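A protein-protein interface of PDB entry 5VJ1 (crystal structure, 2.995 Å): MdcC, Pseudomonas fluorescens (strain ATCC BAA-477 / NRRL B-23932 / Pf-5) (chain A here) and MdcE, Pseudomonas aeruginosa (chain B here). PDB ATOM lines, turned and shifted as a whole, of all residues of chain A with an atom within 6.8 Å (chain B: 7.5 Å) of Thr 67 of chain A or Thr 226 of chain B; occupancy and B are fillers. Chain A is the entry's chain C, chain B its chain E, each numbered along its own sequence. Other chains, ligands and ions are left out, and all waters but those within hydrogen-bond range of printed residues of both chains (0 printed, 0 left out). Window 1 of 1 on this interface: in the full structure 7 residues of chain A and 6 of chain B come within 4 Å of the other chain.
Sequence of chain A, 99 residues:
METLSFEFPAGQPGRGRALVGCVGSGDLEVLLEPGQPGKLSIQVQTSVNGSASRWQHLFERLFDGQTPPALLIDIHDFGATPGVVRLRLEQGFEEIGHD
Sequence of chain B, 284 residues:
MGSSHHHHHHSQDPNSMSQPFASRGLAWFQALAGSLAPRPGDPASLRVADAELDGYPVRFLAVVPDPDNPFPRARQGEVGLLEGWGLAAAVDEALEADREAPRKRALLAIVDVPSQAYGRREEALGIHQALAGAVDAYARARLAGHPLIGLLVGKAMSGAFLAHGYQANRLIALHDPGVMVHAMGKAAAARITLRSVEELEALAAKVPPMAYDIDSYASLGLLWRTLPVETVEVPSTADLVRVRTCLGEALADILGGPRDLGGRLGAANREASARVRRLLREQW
The backbone NH (N) of Thr 226 of chain B lies within hydrogen-bond range of the side-chain hydroxyl (OG1) of Thr 67 of chain A. O of Leu 223 of chain B sits close to O of Gly 65 of chain A, 3.2 Å away.
O of Pro 68 of chain A lies within hydrogen-bond range of N of Gly 11 of chain A (2.9 Å). N of Trp 224 of chain B is in hydrogen-bond range of O of Leu 171 of chain B (2.8 Å). N of Ala 173 of chain B sits at hydrogen-bond distance from O of Arg 225 of chain B, 3.1 Å away. A ring nitrogen (NE2) of His 175 of chain B sits at hydrogen-bond distance from the side-chain carboxylate (OD1) of Asp 215 of chain B (2.9 Å). The backbone NH (N) of His 175 of chain B is in hydrogen-bond range of the backbone carbonyl oxygen (O) of Leu 227 of chain B (2.9 Å).
Among the printed residues, merely in contact across the chains: Thr 67 of chain A with Arg 225 of chain B, Gln 12 of chain A with Pro 228 of chain B, Ala 10 of chain A with Pro 228 of chain B, Gln 12 of chain A with His 175 of chain B, Pro 9 of chain A with Arg 225 of chain B, Gly 11 of chain A with Pro 228 of chain B and Gly 65 of chain A with Trp 224 of chain B.
Of chain B, only Arg 225 and Thr 226 come within 4 Å of Thr 67 of chain A. Thr 226 of chain B touches just one residue of chain A: Thr 67. Printed residues of chain A within 4 Å of His 175 of chain B: Gln 12. Of the printed residues of chain B, Ala 10 of chain A touches Pro 228 (3.3 Å). Of the printed residues of chain B, Gly 11 of chain A touches Pro 228 (3.5 Å). Printed residues of chain A within 4 Å of Pro 228 of chain B: Ala 10, Gly 11 and Gln 12. Of the printed residues of chain A, Arg 225 of chain B touches Pro 9 and Thr 67. Cys 246 of chain B touches none of the printed residues of chain A. The nearest residue of chain B that does not touch Thr 67 of chain A is Trp 224 of chain B (4.1 Å). The nearest residue of chain A that does not touch Thr 226 of chain B is Ala 10 of chain A (4.04 Å).
Of the 17 printed residues of chain B, 6 touch a printed residue of chain A. Along chain B the printed residues that touch a printed residue of chain A span positions 175 to 228. Printed residues of chain A that touch a printed residue of chain B: Pro 9, Ala 10, Gly 11, Gln 12, Gly 65 and Thr 67. Among the printed residues, 9 pairs touch across the chains.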
ATOM      1  N   PRO A   9      -2.043 -35.141   0.447  1.00  0.00           N
ATOM      2  CA  PRO A   9      -0.898 -34.451   1.032  1.00  0.00           C
ATOM      3  C   PRO A   9      -1.293 -33.023   1.397  1.00  0.00           C
ATOM      4  O   PRO A   9      -1.896 -32.314   0.584  1.00  0.00           O
ATOM      5  CB  PRO A   9       0.150 -34.503  -0.090  1.00  0.00           C
ATOM      6  CG  PRO A   9      -0.675 -34.542  -1.332  1.00  0.00           C
ATOM      7  CD  PRO A   9      -1.818 -35.454  -0.975  1.00  0.00           C
ATOM      8  N   ALA A  10      -0.999 -32.636   2.633  1.00  0.00           N
ATOM      9  CA  ALA A  10      -1.338 -31.315   3.129  1.00  0.00           C
ATOM     10  C   ALA A  10      -0.166 -30.690   3.880  1.00  0.00           C
ATOM     11  O   ALA A  10       0.937 -31.254   3.920  1.00  0.00           O
ATOM     12  CB  ALA A  10      -2.563 -31.386   4.017  1.00  0.00           C
ATOM     13  N   GLY A  11      -0.428 -29.526   4.475  1.00  0.00           N
ATOM     14  CA  GLY A  11       0.586 -28.727   5.145  1.00  0.00           C
ATOM     15  C   GLY A  11       0.623 -28.870   6.649  1.00  0.00           C
ATOM     16  O   GLY A  11       0.715 -29.978   7.166  1.00  0.00           O
ATOM     17  N   GLN A  12       0.574 -27.746   7.358  1.00  0.00           N
ATOM     18  CA  GLN A  12       0.559 -27.765   8.819  1.00  0.00           C
ATOM     19  C   GLN A  12      -0.888 -27.819   9.292  1.00  0.00           C
ATOM     20  O   GLN A  12      -1.786 -27.486   8.533  1.00  0.00           O
ATOM     21  CB  GLN A  12       1.283 -26.550   9.376  1.00  0.00           C
ATOM     22  CG  GLN A  12       2.770 -26.531   9.041  1.00  0.00           C
ATOM     23  CD  GLN A  12       3.554 -27.705   9.627  1.00  0.00           C
ATOM     24  OE1 GLN A  12       3.186 -28.260  10.665  1.00  0.00           O
ATOM     25  NE2 GLN A  12       4.656 -28.070   8.967  1.00  0.00           N
ATOM     26  N   PHE A  63      -8.013 -29.318  -4.494  1.00  0.00           N
ATOM     27  CA  PHE A  63      -6.635 -29.228  -3.986  1.00  0.00           C
ATOM     28  C   PHE A  63      -5.522 -29.138  -5.043  1.00  0.00           C
ATOM     29  O   PHE A  63      -4.342 -29.206  -4.698  1.00  0.00           O
ATOM     30  CB  PHE A  63      -6.364 -30.422  -3.080  1.00  0.00           C
ATOM     31  CG  PHE A  63      -7.394 -30.591  -2.018  1.00  0.00           C
ATOM     32  CD1 PHE A  63      -7.939 -31.840  -1.753  1.00  0.00           C
ATOM     33  CD2 PHE A  63      -7.833 -29.492  -1.293  1.00  0.00           C
ATOM     34  CE1 PHE A  63      -8.904 -31.994  -0.781  1.00  0.00           C
ATOM     35  CE2 PHE A  63      -8.795 -29.632  -0.322  1.00  0.00           C
ATOM     36  CZ  PHE A  63      -9.330 -30.891  -0.061  1.00  0.00           C
ATOM     37  N   ASP A  64      -5.900 -28.985  -6.313  1.00  0.00           N
ATOM     38  CA  ASP A  64      -4.945 -28.879  -7.421  1.00  0.00           C
ATOM     39  C   ASP A  64      -4.077 -27.635  -7.258  1.00  0.00           C
ATOM     40  O   ASP A  64      -4.580 -26.516  -7.312  1.00  0.00           O
ATOM     41  CB  ASP A  64      -5.709 -28.839  -8.767  1.00  0.00           C
ATOM     42  CG  ASP A  64      -4.791 -28.643  -9.997  1.00  0.00           C
ATOM     43  OD1 ASP A  64      -5.335 -28.304 -11.080  1.00  0.00           O
ATOM     44  OD2 ASP A  64      -3.549 -28.810  -9.895  1.00  0.00           O
ATOM     45  N   GLY A  65      -2.774 -27.824  -7.089  1.00  0.00           N
ATOM     46  CA  GLY A  65      -1.845 -26.704  -7.023  1.00  0.00           C
ATOM     47  C   GLY A  65      -1.953 -25.774  -5.824  1.00  0.00           C
ATOM     48  O   GLY A  65      -1.307 -24.717  -5.768  1.00  0.00           O
ATOM     49  N   GLN A  66      -2.776 -26.172  -4.867  1.00  0.00           N
ATOM     50  CA  GLN A  66      -2.971 -25.420  -3.642  1.00  0.00           C
ATOM     51  C   GLN A  66      -2.969 -26.477  -2.570  1.00  0.00           C
ATOM     52  O   GLN A  66      -3.864 -27.307  -2.527  1.00  0.00           O
ATOM     53  CB  GLN A  66      -4.294 -24.608  -3.623  1.00  0.00           C
ATOM     54  CG  GLN A  66      -4.933 -24.283  -5.012  1.00  0.00           C
ATOM     55  CD  GLN A  66      -6.388 -23.762  -4.945  1.00  0.00           C
ATOM     56  OE1 GLN A  66      -7.290 -24.469  -4.490  1.00  0.00           O
ATOM     57  NE2 GLN A  66      -6.615 -22.529  -5.417  1.00  0.00           N
ATOM     58  N   THR A  67      -1.923 -26.502  -1.752  1.00  0.00           N
ATOM     59  CA  THR A  67      -1.863 -27.452  -0.645  1.00  0.00           C
ATOM     60  C   THR A  67      -2.699 -26.955   0.523  1.00  0.00           C
ATOM     61  O   THR A  67      -2.516 -25.835   0.999  1.00  0.00           O
ATOM     62  CB  THR A  67      -0.415 -27.715  -0.173  1.00  0.00           C
ATOM     63  OG1 THR A  67       0.359 -28.172  -1.282  1.00  0.00           O
ATOM     64  CG2 THR A  67      -0.385 -28.794   0.892  1.00  0.00           C
ATOM     65  N   PRO A  68      -3.634 -27.791   0.981  1.00  0.00           N
ATOM     66  CA  PRO A  68      -4.553 -27.427   2.055  1.00  0.00           C
ATOM     67  C   PRO A  68      -3.911 -27.550   3.420  1.00  0.00           C
ATOM     68  O   PRO A  68      -2.862 -28.171   3.560  1.00  0.00           O
ATOM     69  CB  PRO A  68      -5.668 -28.456   1.895  1.00  0.00           C
ATOM     70  CG  PRO A  68      -4.925 -29.683   1.475  1.00  0.00           C
ATOM     71  CD  PRO A  68      -3.904 -29.152   0.483  1.00  0.00           C
ATOM     72  N   PRO A  69      -4.546 -26.967   4.433  1.00  0.00           N
ATOM     73  CA  PRO A  69      -4.066 -27.210   5.793  1.00  0.00           C
ATOM     74  C   PRO A  69      -4.330 -28.661   6.160  1.00  0.00           C
ATOM     75  O   PRO A  69      -5.220 -29.274   5.572  1.00  0.00           O
ATOM     76  CB  PRO A  69      -4.919 -26.263   6.639  1.00  0.00           C
ATOM     77  CG  PRO A  69      -6.231 -26.196   5.861  1.00  0.00           C
ATOM     78  CD  PRO A  69      -5.772 -26.142   4.416  1.00  0.00           C
ATOM     79  N   LEU B 171       6.975 -25.030  -8.357  1.00  0.00           N
ATOM     80  CA  LEU B 171       7.718 -24.796  -7.134  1.00  0.00           C
ATOM     81  C   LEU B 171       7.178 -25.654  -5.984  1.00  0.00           C
ATOM     82  O   LEU B 171       5.963 -25.742  -5.776  1.00  0.00           O
ATOM     83  CB  LEU B 171       7.652 -23.328  -6.770  1.00  0.00           C
ATOM     84  CG  LEU B 171       8.474 -22.408  -7.666  1.00  0.00           C
ATOM     85  CD1 LEU B 171       8.199 -20.949  -7.304  1.00  0.00           C
ATOM     86  CD2 LEU B 171       9.965 -22.724  -7.578  1.00  0.00           C
ATOM     87  N   ILE B 172       8.092 -26.272  -5.239  1.00  0.00           N
ATOM     88  CA  ILE B 172       7.766 -27.076  -4.060  1.00  0.00           C
ATOM     89  C   ILE B 172       8.602 -26.598  -2.891  1.00  0.00           C
ATOM     90  O   ILE B 172       9.820 -26.506  -2.993  1.00  0.00           O
ATOM     91  CB  ILE B 172       8.057 -28.591  -4.254  1.00  0.00           C
ATOM     92  CG1 ILE B 172       7.241 -29.183  -5.397  1.00  0.00           C
ATOM     93  CG2 ILE B 172       7.735 -29.340  -2.992  1.00  0.00           C
ATOM     94  CD1 ILE B 172       7.639 -30.598  -5.754  1.00  0.00           C
ATOM     95  N   ALA B 173       7.966 -26.266  -1.785  1.00  0.00           N
ATOM     96  CA  ALA B 173       8.734 -25.822  -0.643  1.00  0.00           C
ATOM     97  C   ALA B 173       8.505 -26.765   0.518  1.00  0.00           C
ATOM     98  O   ALA B 173       7.415 -27.301   0.671  1.00  0.00           O
ATOM     99  CB  ALA B 173       8.364 -24.400  -0.266  1.00  0.00           C
ATOM    100  N   LEU B 174       9.521 -26.958   1.348  1.00  0.00           N
ATOM    101  CA  LEU B 174       9.346 -27.730   2.562  1.00  0.00           C
ATOM    102  C   LEU B 174       8.650 -26.836   3.562  1.00  0.00           C
ATOM    103  O   LEU B 174       9.012 -25.674   3.704  1.00  0.00           O
ATOM    104  CB  LEU B 174      10.686 -28.174   3.131  1.00  0.00           C
ATOM    105  CG  LEU B 174      11.610 -29.077   2.326  1.00  0.00           C
ATOM    106  CD1 LEU B 174      12.850 -29.284   3.149  1.00  0.00           C
ATOM    107  CD2 LEU B 174      10.944 -30.400   1.989  1.00  0.00           C
ATOM    108  N   HIS B 175       7.645 -27.344   4.259  1.00  0.00           N
ATOM    109  CA  HIS B 175       7.034 -26.494   5.265  1.00  0.00           C
ATOM    110  C   HIS B 175       7.850 -26.504   6.545  1.00  0.00           C
ATOM    111  O   HIS B 175       7.781 -27.449   7.341  1.00  0.00           O
ATOM    112  CB  HIS B 175       5.606 -26.910   5.571  1.00  0.00           C
ATOM    113  CG  HIS B 175       4.784 -25.768   6.093  1.00  0.00           C
ATOM    114  ND1 HIS B 175       5.218 -24.967   7.121  1.00  0.00           N
ATOM    115  CD2 HIS B 175       3.585 -25.287   5.709  1.00  0.00           C
ATOM    116  CE1 HIS B 175       4.318 -24.037   7.366  1.00  0.00           C
ATOM    117  NE2 HIS B 175       3.306 -24.210   6.517  1.00  0.00           N
ATOM    118  N   ASP B 176       8.577 -25.411   6.748  1.00  0.00           N
ATOM    119  CA  ASP B 176       9.505 -25.268   7.862  1.00  0.00           C
ATOM    120  C   ASP B 176      10.028 -23.831   7.985  1.00  0.00           C
ATOM    121  O   ASP B 176      10.409 -23.206   6.991  1.00  0.00           O
ATOM    122  CB  ASP B 176      10.687 -26.241   7.694  1.00  0.00           C
ATOM    123  CG  ASP B 176      11.795 -26.020   8.733  1.00  0.00           C
ATOM    124  OD1 ASP B 176      11.609 -26.420   9.907  1.00  0.00           O
ATOM    125  OD2 ASP B 176      12.860 -25.463   8.371  1.00  0.00           O
ATOM    126  N   ILE B 214       7.265 -18.929   4.898  1.00  0.00           N
ATOM    127  CA  ILE B 214       6.769 -19.741   3.806  1.00  0.00           C
ATOM    128  C   ILE B 214       5.231 -19.827   3.785  1.00  0.00           C
ATOM    129  O   ILE B 214       4.641 -20.234   2.775  1.00  0.00           O
ATOM    130  CB  ILE B 214       7.390 -21.172   3.889  1.00  0.00           C
ATOM    131  CG1 ILE B 214       7.169 -21.951   2.598  1.00  0.00           C
ATOM    132  CG2 ILE B 214       6.841 -21.931   5.075  1.00  0.00           C
ATOM    133  CD1 ILE B 214       7.760 -21.268   1.386  1.00  0.00           C
ATOM    134  N   ASP B 215       4.575 -19.460   4.884  1.00  0.00           N
ATOM    135  CA  ASP B 215       3.113 -19.485   4.897  1.00  0.00           C
ATOM    136  C   ASP B 215       2.592 -18.305   4.099  1.00  0.00           C
ATOM    137  O   ASP B 215       1.637 -18.424   3.314  1.00  0.00           O
ATOM    138  CB  ASP B 215       2.563 -19.446   6.308  1.00  0.00           C
ATOM    139  CG  ASP B 215       2.556 -20.806   6.945  1.00  0.00           C
ATOM    140  OD1 ASP B 215       1.864 -21.694   6.394  1.00  0.00           O
ATOM    141  OD2 ASP B 215       3.247 -20.997   7.975  1.00  0.00           O
ATOM    142  N   TYR B 217       4.324 -16.851   1.806  1.00  0.00           N
ATOM    143  CA  TYR B 217       4.677 -17.074   0.419  1.00  0.00           C
ATOM    144  C   TYR B 217       3.585 -17.922  -0.203  1.00  0.00           C
ATOM    145  O   TYR B 217       3.163 -17.685  -1.318  1.00  0.00           O
ATOM    146  CB  TYR B 217       6.040 -17.744   0.255  1.00  0.00           C
ATOM    147  CG  TYR B 217       6.488 -17.761  -1.190  1.00  0.00           C
ATOM    148  CD1 TYR B 217       6.609 -16.577  -1.892  1.00  0.00           C
ATOM    149  CD2 TYR B 217       6.785 -18.948  -1.853  1.00  0.00           C
ATOM    150  CE1 TYR B 217       7.007 -16.566  -3.210  1.00  0.00           C
ATOM    151  CE2 TYR B 217       7.192 -18.941  -3.175  1.00  0.00           C
ATOM    152  CZ  TYR B 217       7.296 -17.750  -3.844  1.00  0.00           C
ATOM    153  OH  TYR B 217       7.681 -17.731  -5.154  1.00  0.00           O
ATOM    154  N   ALA B 218       3.140 -18.934   0.520  1.00  0.00           N
ATOM    155  CA  ALA B 218       2.156 -19.853  -0.027  1.00  0.00           C
ATOM    156  C   ALA B 218       0.877 -19.119  -0.438  1.00  0.00           C
ATOM    157  O   ALA B 218       0.261 -19.452  -1.451  1.00  0.00           O
ATOM    158  CB  ALA B 218       1.851 -20.968   0.985  1.00  0.00           C
ATOM    159  N   LEU B 223       3.388 -21.515  -5.003  1.00  0.00           N
ATOM    160  CA  LEU B 223       3.868 -22.843  -4.714  1.00  0.00           C
ATOM    161  C   LEU B 223       2.843 -23.839  -5.213  1.00  0.00           C
ATOM    162  O   LEU B 223       1.643 -23.634  -5.036  1.00  0.00           O
ATOM    163  CB  LEU B 223       4.136 -23.004  -3.223  1.00  0.00           C
ATOM    164  CG  LEU B 223       5.422 -22.348  -2.714  1.00  0.00           C
ATOM    165  CD1 LEU B 223       5.528 -22.497  -1.227  1.00  0.00           C
ATOM    166  CD2 LEU B 223       6.625 -22.966  -3.367  1.00  0.00           C
ATOM    167  N   TRP B 224       3.321 -24.876  -5.905  1.00  0.00           N
ATOM    168  CA  TRP B 224       2.460 -25.948  -6.405  1.00  0.00           C
ATOM    169  C   TRP B 224       2.149 -26.917  -5.276  1.00  0.00           C
ATOM    170  O   TRP B 224       1.151 -27.657  -5.316  1.00  0.00           O
ATOM    171  CB  TRP B 224       3.103 -26.687  -7.577  1.00  0.00           C
ATOM    172  CG  TRP B 224       2.227 -27.786  -8.111  1.00  0.00           C
ATOM    173  CD1 TRP B 224       1.107 -27.650  -8.877  1.00  0.00           C
ATOM    174  CD2 TRP B 224       2.379 -29.201  -7.855  1.00  0.00           C
ATOM    175  NE1 TRP B 224       0.566 -28.892  -9.143  1.00  0.00           N
ATOM    176  CE2 TRP B 224       1.312 -29.838  -8.538  1.00  0.00           C
ATOM    177  CE3 TRP B 224       3.297 -29.961  -7.141  1.00  0.00           C
ATOM    178  CZ2 TRP B 224       1.177 -31.230  -8.504  1.00  0.00           C
ATOM    179  CZ3 TRP B 224       3.148 -31.324  -7.124  1.00  0.00           C
ATOM    180  CH2 TRP B 224       2.096 -31.947  -7.799  1.00  0.00           C
ATOM    181  N   ARG B 225       3.023 -26.913  -4.274  1.00  0.00           N
ATOM    182  CA  ARG B 225       2.830 -27.725  -3.077  1.00  0.00           C
ATOM    183  C   ARG B 225       3.868 -27.442  -2.019  1.00  0.00           C
ATOM    184  O   ARG B 225       5.044 -27.250  -2.305  1.00  0.00           O
ATOM    185  CB  ARG B 225       2.844 -29.220  -3.398  1.00  0.00           C
ATOM    186  CG  ARG B 225       2.376 -30.062  -2.229  1.00  0.00           C
ATOM    187  CD  ARG B 225       2.443 -31.542  -2.500  1.00  0.00           C
ATOM    188  NE  ARG B 225       1.661 -31.900  -3.673  1.00  0.00           N
ATOM    189  CZ  ARG B 225       1.503 -33.143  -4.102  1.00  0.00           C
ATOM    190  NH1 ARG B 225       2.076 -34.142  -3.437  1.00  0.00           N
ATOM    191  NH2 ARG B 225       0.777 -33.384  -5.190  1.00  0.00           N
ATOM    192  N   THR B 226       3.391 -27.438  -0.784  1.00  0.00           N
ATOM    193  CA  THR B 226       4.222 -27.340   0.393  1.00  0.00           C
ATOM    194  C   THR B 226       4.081 -28.682   1.066  1.00  0.00           C
ATOM    195  O   THR B 226       2.981 -29.231   1.086  1.00  0.00           O
ATOM    196  CB  THR B 226       3.748 -26.245   1.346  1.00  0.00           C
ATOM    197  OG1 THR B 226       2.346 -26.407   1.578  1.00  0.00           O
ATOM    198  CG2 THR B 226       3.974 -24.899   0.744  1.00  0.00           C
ATOM    199  N   LEU B 227       5.163 -29.225   1.612  1.00  0.00           N
ATOM    200  CA  LEU B 227       5.052 -30.469   2.357  1.00  0.00           C
ATOM    201  C   LEU B 227       5.991 -30.416   3.533  1.00  0.00           C
ATOM    202  O   LEU B 227       7.163 -30.101   3.381  1.00  0.00           O
ATOM    203  CB  LEU B 227       5.325 -31.683   1.467  1.00  0.00           C
ATOM    204  CG  LEU B 227       6.641 -31.821   0.711  1.00  0.00           C
ATOM    205  CD1 LEU B 227       7.728 -32.501   1.548  1.00  0.00           C
ATOM    206  CD2 LEU B 227       6.375 -32.581  -0.560  1.00  0.00           C
ATOM    207  N   PRO B 228       5.439 -30.647   4.728  1.00  0.00           N
ATOM    208  CA  PRO B 228       6.188 -30.642   5.987  1.00  0.00           C
ATOM    209  C   PRO B 228       7.013 -31.907   6.152  1.00  0.00           C
ATOM    210  O   PRO B 228       6.677 -32.926   5.537  1.00  0.00           O
ATOM    211  CB  PRO B 228       5.083 -30.536   7.044  1.00  0.00           C
ATOM    212  CG  PRO B 228       3.907 -31.184   6.402  1.00  0.00           C
ATOM    213  CD  PRO B 228       3.988 -30.787   4.953  1.00  0.00           C
ATOM    214  N   CYS B 246       6.572 -36.703  -4.241  1.00  0.00           N
ATOM    215  CA  CYS B 246       6.040 -35.410  -4.597  1.00  0.00           C
ATOM    216  C   CYS B 246       6.631 -34.943  -5.916  1.00  0.00           C
ATOM    217  O   CYS B 246       5.912 -34.453  -6.802  1.00  0.00           O
ATOM    218  CB  CYS B 246       6.323 -34.394  -3.499  1.00  0.00           C
ATOM    219  SG  CYS B 246       5.631 -32.748  -3.887  1.00  0.00           S
